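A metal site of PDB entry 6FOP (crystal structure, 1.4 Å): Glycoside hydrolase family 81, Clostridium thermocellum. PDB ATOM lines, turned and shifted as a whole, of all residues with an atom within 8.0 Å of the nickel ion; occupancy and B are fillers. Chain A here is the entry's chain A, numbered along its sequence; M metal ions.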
ATOM      1  N   TYR A 547      -8.904  27.035 -31.458  1.00  0.00           N
ATOM      2  CA  TYR A 547      -8.296  25.722 -31.562  1.00  0.00           C
ATOM      3  C   TYR A 547      -7.842  25.335 -30.159  1.00  0.00           C
ATOM      4  O   TYR A 547      -7.197  26.110 -29.459  1.00  0.00           O
ATOM      5  CB  TYR A 547      -7.156  25.743 -32.583  1.00  0.00           C
ATOM      6  CG  TYR A 547      -6.430  24.427 -32.743  1.00  0.00           C
ATOM      7  CD1 TYR A 547      -7.063  23.343 -33.278  1.00  0.00           C
ATOM      8  CD2 TYR A 547      -5.099  24.293 -32.369  1.00  0.00           C
ATOM      9  CE1 TYR A 547      -6.423  22.137 -33.454  1.00  0.00           C
ATOM     10  CE2 TYR A 547      -4.432  23.088 -32.520  1.00  0.00           C
ATOM     11  CZ  TYR A 547      -5.089  22.020 -33.066  1.00  0.00           C
ATOM     12  OH  TYR A 547      -4.486  20.813 -33.221  1.00  0.00           O
ATOM     13  N   GLY A 548      -8.197  24.132 -29.736  1.00  0.00           N
ATOM     14  CA  GLY A 548      -8.050  23.725 -28.339  1.00  0.00           C
ATOM     15  C   GLY A 548      -6.751  23.075 -27.912  1.00  0.00           C
ATOM     16  O   GLY A 548      -6.720  22.368 -26.899  1.00  0.00           O
ATOM     17  N   HIS A 549      -5.665  23.293 -28.642  1.00  0.00           N
ATOM     18  CA  HIS A 549      -4.408  22.593 -28.425  1.00  0.00           C
ATOM     19  C   HIS A 549      -3.246  23.515 -28.751  1.00  0.00           C
ATOM     20  O   HIS A 549      -3.398  24.447 -29.549  1.00  0.00           O
ATOM     21  CB  HIS A 549      -4.362  21.322 -29.295  1.00  0.00           C
ATOM     22  CG  HIS A 549      -5.580  20.456 -29.185  1.00  0.00           C
ATOM     23  ND1 HIS A 549      -5.711  19.489 -28.209  1.00  0.00           N
ATOM     24  CD2 HIS A 549      -6.757  20.494 -29.845  1.00  0.00           C
ATOM     25  CE1 HIS A 549      -6.897  18.938 -28.305  1.00  0.00           C
ATOM     26  NE2 HIS A 549      -7.561  19.537 -29.289  1.00  0.00           N
ATOM     27  N   ASN A 550      -2.062  23.170 -28.228  1.00  0.00           N
ATOM     28  CA  ASN A 550      -0.801  23.837 -28.517  1.00  0.00           C
ATOM     29  C   ASN A 550       0.033  23.138 -29.612  1.00  0.00           C
ATOM     30  O   ASN A 550       1.193  23.493 -29.826  1.00  0.00           O
ATOM     31  CB  ASN A 550       0.017  24.042 -27.238  1.00  0.00           C
ATOM     32  CG  ASN A 550       0.543  22.743 -26.621  1.00  0.00           C
ATOM     33  OD1 ASN A 550       0.678  21.711 -27.276  1.00  0.00           O
ATOM     34  ND2 ASN A 550       0.771  22.795 -25.313  1.00  0.00           N
ATOM     35  N   TYR A 551      -0.594  22.190 -30.285  1.00  0.00           N
ATOM     36  CA  TYR A 551       0.051  21.265 -31.201  1.00  0.00           C
ATOM     37  C   TYR A 551      -1.006  20.823 -32.210  1.00  0.00           C
ATOM     38  O   TYR A 551      -2.130  20.584 -31.823  1.00  0.00           O
ATOM     39  CB  TYR A 551       0.545  20.058 -30.416  1.00  0.00           C
ATOM     40  CG  TYR A 551       0.848  18.802 -31.230  1.00  0.00           C
ATOM     41  CD1 TYR A 551       1.861  18.827 -32.218  1.00  0.00           C
ATOM     42  CD2 TYR A 551       0.158  17.631 -31.030  1.00  0.00           C
ATOM     43  CE1 TYR A 551       2.149  17.691 -32.958  1.00  0.00           C
ATOM     44  CE2 TYR A 551       0.444  16.504 -31.759  1.00  0.00           C
ATOM     45  CZ  TYR A 551       1.461  16.527 -32.717  1.00  0.00           C
ATOM     46  OH  TYR A 551       1.766  15.401 -33.414  1.00  0.00           O
ATOM     47  N   ALA A 552      -0.601  20.759 -33.486  1.00  0.00           N
ATOM     48  CA  ALA A 552      -1.407  20.120 -34.528  1.00  0.00           C
ATOM     49  C   ALA A 552      -0.646  18.905 -35.011  1.00  0.00           C
ATOM     50  O   ALA A 552       0.517  19.010 -35.410  1.00  0.00           O
ATOM     51  CB  ALA A 552      -1.660  21.074 -35.700  1.00  0.00           C
ATOM     52  N   SER A 553      -1.312  17.752 -35.007  1.00  0.00           N
ATOM     53  CA  SER A 553      -0.698  16.508 -35.500  1.00  0.00           C
ATOM     54  C   SER A 553      -0.796  16.315 -37.007  1.00  0.00           C
ATOM     55  O   SER A 553       0.048  15.611 -37.566  1.00  0.00           O
ATOM     56  CB  SER A 553      -1.286  15.308 -34.761  1.00  0.00           C
ATOM     57  OG  SER A 553      -2.694  15.340 -34.753  1.00  0.00           O
ATOM     58  N   HIS A 562      -5.874  17.945 -34.470  1.00  0.00           N
ATOM     59  CA  HIS A 562      -5.249  17.141 -33.429  1.00  0.00           C
ATOM     60  C   HIS A 562      -5.792  15.704 -33.525  1.00  0.00           C
ATOM     61  O   HIS A 562      -6.256  15.121 -32.549  1.00  0.00           O
ATOM     62  CB  HIS A 562      -5.551  17.813 -32.108  1.00  0.00           C
ATOM     63  CG  HIS A 562      -4.780  17.306 -30.925  1.00  0.00           C
ATOM     64  ND1 HIS A 562      -5.181  16.220 -30.172  1.00  0.00           N
ATOM     65  CD2 HIS A 562      -3.707  17.820 -30.296  1.00  0.00           C
ATOM     66  CE1 HIS A 562      -4.360  16.070 -29.140  1.00  0.00           C
ATOM     67  NE2 HIS A 562      -3.476  17.042 -29.179  1.00  0.00           N
ATOM     68  N   ASN A 570      -3.511  10.013 -26.973  1.00  0.00           N
ATOM     69  CA  ASN A 570      -2.939  11.336 -27.167  1.00  0.00           C
ATOM     70  C   ASN A 570      -1.404  11.336 -27.089  1.00  0.00           C
ATOM     71  O   ASN A 570      -0.750  12.199 -27.694  1.00  0.00           O
ATOM     72  CB  ASN A 570      -3.591  12.377 -26.237  1.00  0.00           C
ATOM     73  CG  ASN A 570      -5.029  12.635 -26.607  1.00  0.00           C
ATOM     74  OD1 ASN A 570      -5.990  12.094 -26.000  1.00  0.00           O
ATOM     75  ND2 ASN A 570      -5.205  13.377 -27.644  1.00  0.00           N
ATOM     76  N   SER A 571      -0.831  10.345 -26.407  1.00  0.00           N
ATOM     77  CA  SER A 571       0.608  10.129 -26.498  1.00  0.00           C
ATOM     78  C   SER A 571       1.046   9.783 -27.917  1.00  0.00           C
ATOM     79  O   SER A 571       2.054  10.329 -28.414  1.00  0.00           O
ATOM     80  CB  SER A 571       1.062   9.084 -25.502  1.00  0.00           C
ATOM     81  OG  SER A 571       2.458   8.900 -25.621  1.00  0.00           O
ATOM     82  N   LYS A 573      -0.688  10.583 -30.607  1.00  0.00           N
ATOM     83  CA  LYS A 573      -0.950  11.744 -31.422  1.00  0.00           C
ATOM     84  C   LYS A 573       0.211  12.732 -31.375  1.00  0.00           C
ATOM     85  O   LYS A 573       0.609  13.289 -32.410  1.00  0.00           O
ATOM     86  CB  LYS A 573      -2.255  12.429 -31.035  1.00  0.00           C
ATOM     87  CG  LYS A 573      -3.494  11.602 -31.297  1.00  0.00           C
ATOM     88  CD  LYS A 573      -4.770  12.342 -30.994  1.00  0.00           C
ATOM     89  CE  LYS A 573      -5.970  11.419 -31.094  1.00  0.00           C
ATOM     90  NZ  LYS A 573      -7.255  12.124 -30.932  1.00  0.00           N
ATOM     91  N   HIS A 574       0.764  12.965 -30.188  1.00  0.00           N
ATOM     92  CA  HIS A 574       1.949  13.837 -30.032  1.00  0.00           C
ATOM     93  C   HIS A 574       3.221  13.187 -30.612  1.00  0.00           C
ATOM     94  O   HIS A 574       4.014  13.844 -31.296  1.00  0.00           O
ATOM     95  CB  HIS A 574       2.120  14.181 -28.548  1.00  0.00           C
ATOM     96  CG  HIS A 574       1.209  15.279 -28.086  1.00  0.00           C
ATOM     97  ND1 HIS A 574       1.680  16.479 -27.635  1.00  0.00           N
ATOM     98  CD2 HIS A 574      -0.126  15.371 -28.082  1.00  0.00           C
ATOM     99  CE1 HIS A 574       0.675  17.266 -27.347  1.00  0.00           C
ATOM    100  NE2 HIS A 574      -0.434  16.618 -27.596  1.00  0.00           N
ATOM    101  N   TYR A 594       8.397  24.931 -24.364  1.00  0.00           N
ATOM    102  CA  TYR A 594       7.395  24.287 -25.204  1.00  0.00           C
ATOM    103  C   TYR A 594       7.403  22.774 -25.002  1.00  0.00           C
ATOM    104  O   TYR A 594       6.352  22.145 -24.985  1.00  0.00           O
ATOM    105  CB  TYR A 594       7.557  24.628 -26.709  1.00  0.00           C
ATOM    106  CG  TYR A 594       6.481  23.956 -27.534  1.00  0.00           C
ATOM    107  CD1 TYR A 594       5.169  24.441 -27.532  1.00  0.00           C
ATOM    108  CD2 TYR A 594       6.743  22.791 -28.255  1.00  0.00           C
ATOM    109  CE1 TYR A 594       4.161  23.778 -28.229  1.00  0.00           C
ATOM    110  CE2 TYR A 594       5.743  22.114 -28.957  1.00  0.00           C
ATOM    111  CZ  TYR A 594       4.443  22.643 -28.961  1.00  0.00           C
ATOM    112  OH  TYR A 594       3.462  21.986 -29.647  1.00  0.00           O
ATOM    113  N   GLN A 597       5.263  22.312 -21.999  1.00  0.00           N
ATOM    114  CA  GLN A 597       3.858  22.578 -22.312  1.00  0.00           C
ATOM    115  C   GLN A 597       3.232  21.475 -23.164  1.00  0.00           C
ATOM    116  O   GLN A 597       2.073  21.094 -22.975  1.00  0.00           O
ATOM    117  CB  GLN A 597       3.705  23.904 -23.052  1.00  0.00           C
ATOM    118  CG  GLN A 597       3.985  25.150 -22.237  1.00  0.00           C
ATOM    119  CD  GLN A 597       3.960  26.413 -23.101  1.00  0.00           C
ATOM    120  OE1 GLN A 597       4.437  26.434 -24.236  1.00  0.00           O
ATOM    121  NE2 GLN A 597       3.376  27.472 -22.570  1.00  0.00           N
ATOM    122  N   ASN A 598       3.979  21.030 -24.190  1.00  0.00           N
ATOM    123  CA  ASN A 598       3.501  19.994 -25.101  1.00  0.00           C
ATOM    124  C   ASN A 598       3.280  18.681 -24.335  1.00  0.00           C
ATOM    125  O   ASN A 598       2.221  18.036 -24.445  1.00  0.00           O
ATOM    126  CB  ASN A 598       4.470  19.874 -26.297  1.00  0.00           C
ATOM    127  CG  ASN A 598       4.099  18.774 -27.242  1.00  0.00           C
ATOM    128  OD1 ASN A 598       4.095  17.589 -26.894  1.00  0.00           O
ATOM    129  ND2 ASN A 598       3.839  19.138 -28.509  1.00  0.00           N
ATOM    130  N   TYR A 599       4.285  18.269 -23.567  1.00  0.00           N
ATOM    131  CA  TYR A 599       4.183  17.067 -22.753  1.00  0.00           C
ATOM    132  C   TYR A 599       3.059  17.135 -21.736  1.00  0.00           C
ATOM    133  O   TYR A 599       2.294  16.159 -21.601  1.00  0.00           O
ATOM    134  CB  TYR A 599       5.540  16.807 -22.094  1.00  0.00           C
ATOM    135  CG  TYR A 599       5.621  15.591 -21.209  1.00  0.00           C
ATOM    136  CD1 TYR A 599       5.983  14.347 -21.714  1.00  0.00           C
ATOM    137  CD2 TYR A 599       5.422  15.700 -19.831  1.00  0.00           C
ATOM    138  CE1 TYR A 599       6.086  13.243 -20.870  1.00  0.00           C
ATOM    139  CE2 TYR A 599       5.564  14.614 -18.993  1.00  0.00           C
ATOM    140  CZ  TYR A 599       5.847  13.376 -19.530  1.00  0.00           C
ATOM    141  OH  TYR A 599       5.995  12.285 -18.686  1.00  0.00           O
ATOM    142  N   GLU A 600       2.917  18.285 -21.067  1.00  0.00           N
ATOM    143  CA  GLU A 600       1.842  18.433 -20.077  1.00  0.00           C
ATOM    144  C   GLU A 600       0.451  18.445 -20.727  1.00  0.00           C
ATOM    145  O   GLU A 600      -0.484  17.885 -20.164  1.00  0.00           O
ATOM    146  CB  GLU A 600       2.059  19.656 -19.184  1.00  0.00           C
ATOM    147  CG  GLU A 600       3.267  19.521 -18.234  1.00  0.00           C
ATOM    148  CD  GLU A 600       3.129  18.425 -17.163  1.00  0.00           C
ATOM    149  OE1 GLU A 600       2.007  18.155 -16.703  1.00  0.00           O
ATOM    150  OE2 GLU A 600       4.161  17.824 -16.790  1.00  0.00           O
ATOM    151  N   GLU A 601       0.346  19.029 -21.934  1.00  0.00           N
ATOM    152  CA  GLU A 601      -0.932  18.928 -22.650  1.00  0.00           C
ATOM    153  C   GLU A 601      -1.262  17.463 -22.945  1.00  0.00           C
ATOM    154  O   GLU A 601      -2.385  17.011 -22.773  1.00  0.00           O
ATOM    155  CB  GLU A 601      -0.893  19.689 -23.980  1.00  0.00           C
ATOM    156  CG  GLU A 601      -2.063  19.350 -24.895  1.00  0.00           C
ATOM    157  CD  GLU A 601      -2.107  20.081 -26.218  1.00  0.00           C
ATOM    158  OE1 GLU A 601      -2.218  21.308 -26.199  1.00  0.00           O
ATOM    159  OE2 GLU A 601      -2.040  19.423 -27.279  1.00  0.00           O
ATOM    160  N   MET A 602      -0.263  16.739 -23.444  1.00  0.00           N
ATOM    161  CA  MET A 602      -0.427  15.316 -23.753  1.00  0.00           C
ATOM    162  C   MET A 602      -0.926  14.518 -22.526  1.00  0.00           C
ATOM    163  O   MET A 602      -1.867  13.721 -22.642  1.00  0.00           O
ATOM    164  CB  MET A 602       0.911  14.770 -24.321  1.00  0.00           C
ATOM    165  CG  MET A 602       0.954  13.282 -24.614  1.00  0.00           C
ATOM    166  SD  MET A 602       1.272  12.230 -23.189  1.00  0.00           S
ATOM    167  CE  MET A 602       2.872  12.841 -22.696  1.00  0.00           C
ATOM    168  N   LEU A 603      -0.343  14.772 -21.367  1.00  0.00           N
ATOM    169  CA  LEU A 603      -0.774  14.107 -20.140  1.00  0.00           C
ATOM    170  C   LEU A 603      -2.232  14.432 -19.790  1.00  0.00           C
ATOM    171  O   LEU A 603      -3.017  13.526 -19.448  1.00  0.00           O
ATOM    172  CB  LEU A 603       0.127  14.486 -18.958  1.00  0.00           C
ATOM    173  CG  LEU A 603       1.572  14.023 -18.975  1.00  0.00           C
ATOM    174  CD1 LEU A 603       2.231  14.456 -17.678  1.00  0.00           C
ATOM    175  CD2 LEU A 603       1.666  12.512 -19.154  1.00  0.00           C
ATOM    176  N   ARG A 604      -2.567  15.723 -19.856  1.00  0.00           N
ATOM    177  CA  ARG A 604      -3.937  16.140 -19.580  1.00  0.00           C
ATOM    178  C   ARG A 604      -4.937  15.454 -20.497  1.00  0.00           C
ATOM    179  O   ARG A 604      -5.995  14.994 -20.091  1.00  0.00           O
ATOM    180  CB  ARG A 604      -4.083  17.656 -19.704  1.00  0.00           C
ATOM    181  CG  ARG A 604      -3.468  18.452 -18.574  1.00  0.00           C
ATOM    182  CD  ARG A 604      -4.028  19.863 -18.568  1.00  0.00           C
ATOM    183  NE  ARG A 604      -3.736  20.572 -19.815  1.00  0.00           N
ATOM    184  CZ  ARG A 604      -2.574  21.164 -20.121  1.00  0.00           C
ATOM    185  NH1 ARG A 604      -1.552  21.162 -19.266  1.00  0.00           N
ATOM    186  NH2 ARG A 604      -2.430  21.782 -21.281  1.00  0.00           N
ATOM    187  N   GLU A 605      -4.579  15.391 -21.775  1.00  0.00           N
ATOM    188  CA  GLU A 605      -5.440  14.774 -22.773  1.00  0.00           C
ATOM    189  C   GLU A 605      -5.572  13.268 -22.589  1.00  0.00           C
ATOM    190  O   GLU A 605      -6.619  12.701 -22.881  1.00  0.00           O
ATOM    191  CB  GLU A 605      -4.960  15.122 -24.192  1.00  0.00           C
ATOM    192  CG  GLU A 605      -5.080  16.614 -24.468  1.00  0.00           C
ATOM    193  CD  GLU A 605      -4.326  17.108 -25.677  1.00  0.00           C
ATOM    194  OE1 GLU A 605      -3.308  16.498 -26.125  1.00  0.00           O
ATOM    195  OE2 GLU A 605      -4.682  18.193 -26.154  1.00  0.00           O
ATOM    196  N   CYS A 606      -4.492  12.614 -22.143  1.00  0.00           N
ATOM    197  CA  CYS A 606      -4.556  11.185 -21.822  1.00  0.00           C
ATOM    198  C   CYS A 606      -5.298  10.897 -20.520  1.00  0.00           C
ATOM    199  O   CYS A 606      -5.727   9.778 -20.303  1.00  0.00           O
ATOM    200  CB  CYS A 606      -3.145  10.568 -21.740  1.00  0.00           C
ATOM    201  SG  CYS A 606      -2.272  10.515 -23.309  1.00  0.00           S
HETATM  202 NI    NI M   1      -2.325  17.456 -27.504  1.00  0.00          NI
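ND1 of His 549 lies within hydrogen-bond range of OE2 of Glu 605 (2.6 Å). The side-chain amide oxygen of Asn 570 lies close to the backbone carbonyl oxygen of Glu 605, at 3.2 Å. The backbone NH (N) of Asn 550 lies within hydrogen-bond range of the side-chain carboxylate (OE1) of Glu 601, 2.8 Å away. The side-chain hydroxyl (OH) of Tyr 551 is in hydrogen-bond range of the backbone carbonyl oxygen (O) of His 574, 3.5 Å away. A ring nitrogen (ND1) of His 574 lies within hydrogen-bond range of the side-chain amide oxygen (OD1) of Asn 598 (2.8 Å). A ring nitrogen (ND1) of His 549 lies close to a ring nitrogen (NE2) of His 562. N of His 562 lies close to OH of Tyr 547, at 3.4 Å.
Of the 23 residues printed, 4 come within 4 Å of the nickel ion. The nearest printed residue that does not touch the nickel ion is His 549 (4.01 Å).
The nickel ion is bound by OE1 of Glu 605. The nickel ion is bound by OE2 of Glu 601. NE2 of His 574 binds the nickel ion (2.1 Å). NE2 of His 562 binds the nickel ion (2.1 Å). Slightly farther from the nickel ion lies the side-chain carboxylate (OE2) of Glu 605 (2.8 Å).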
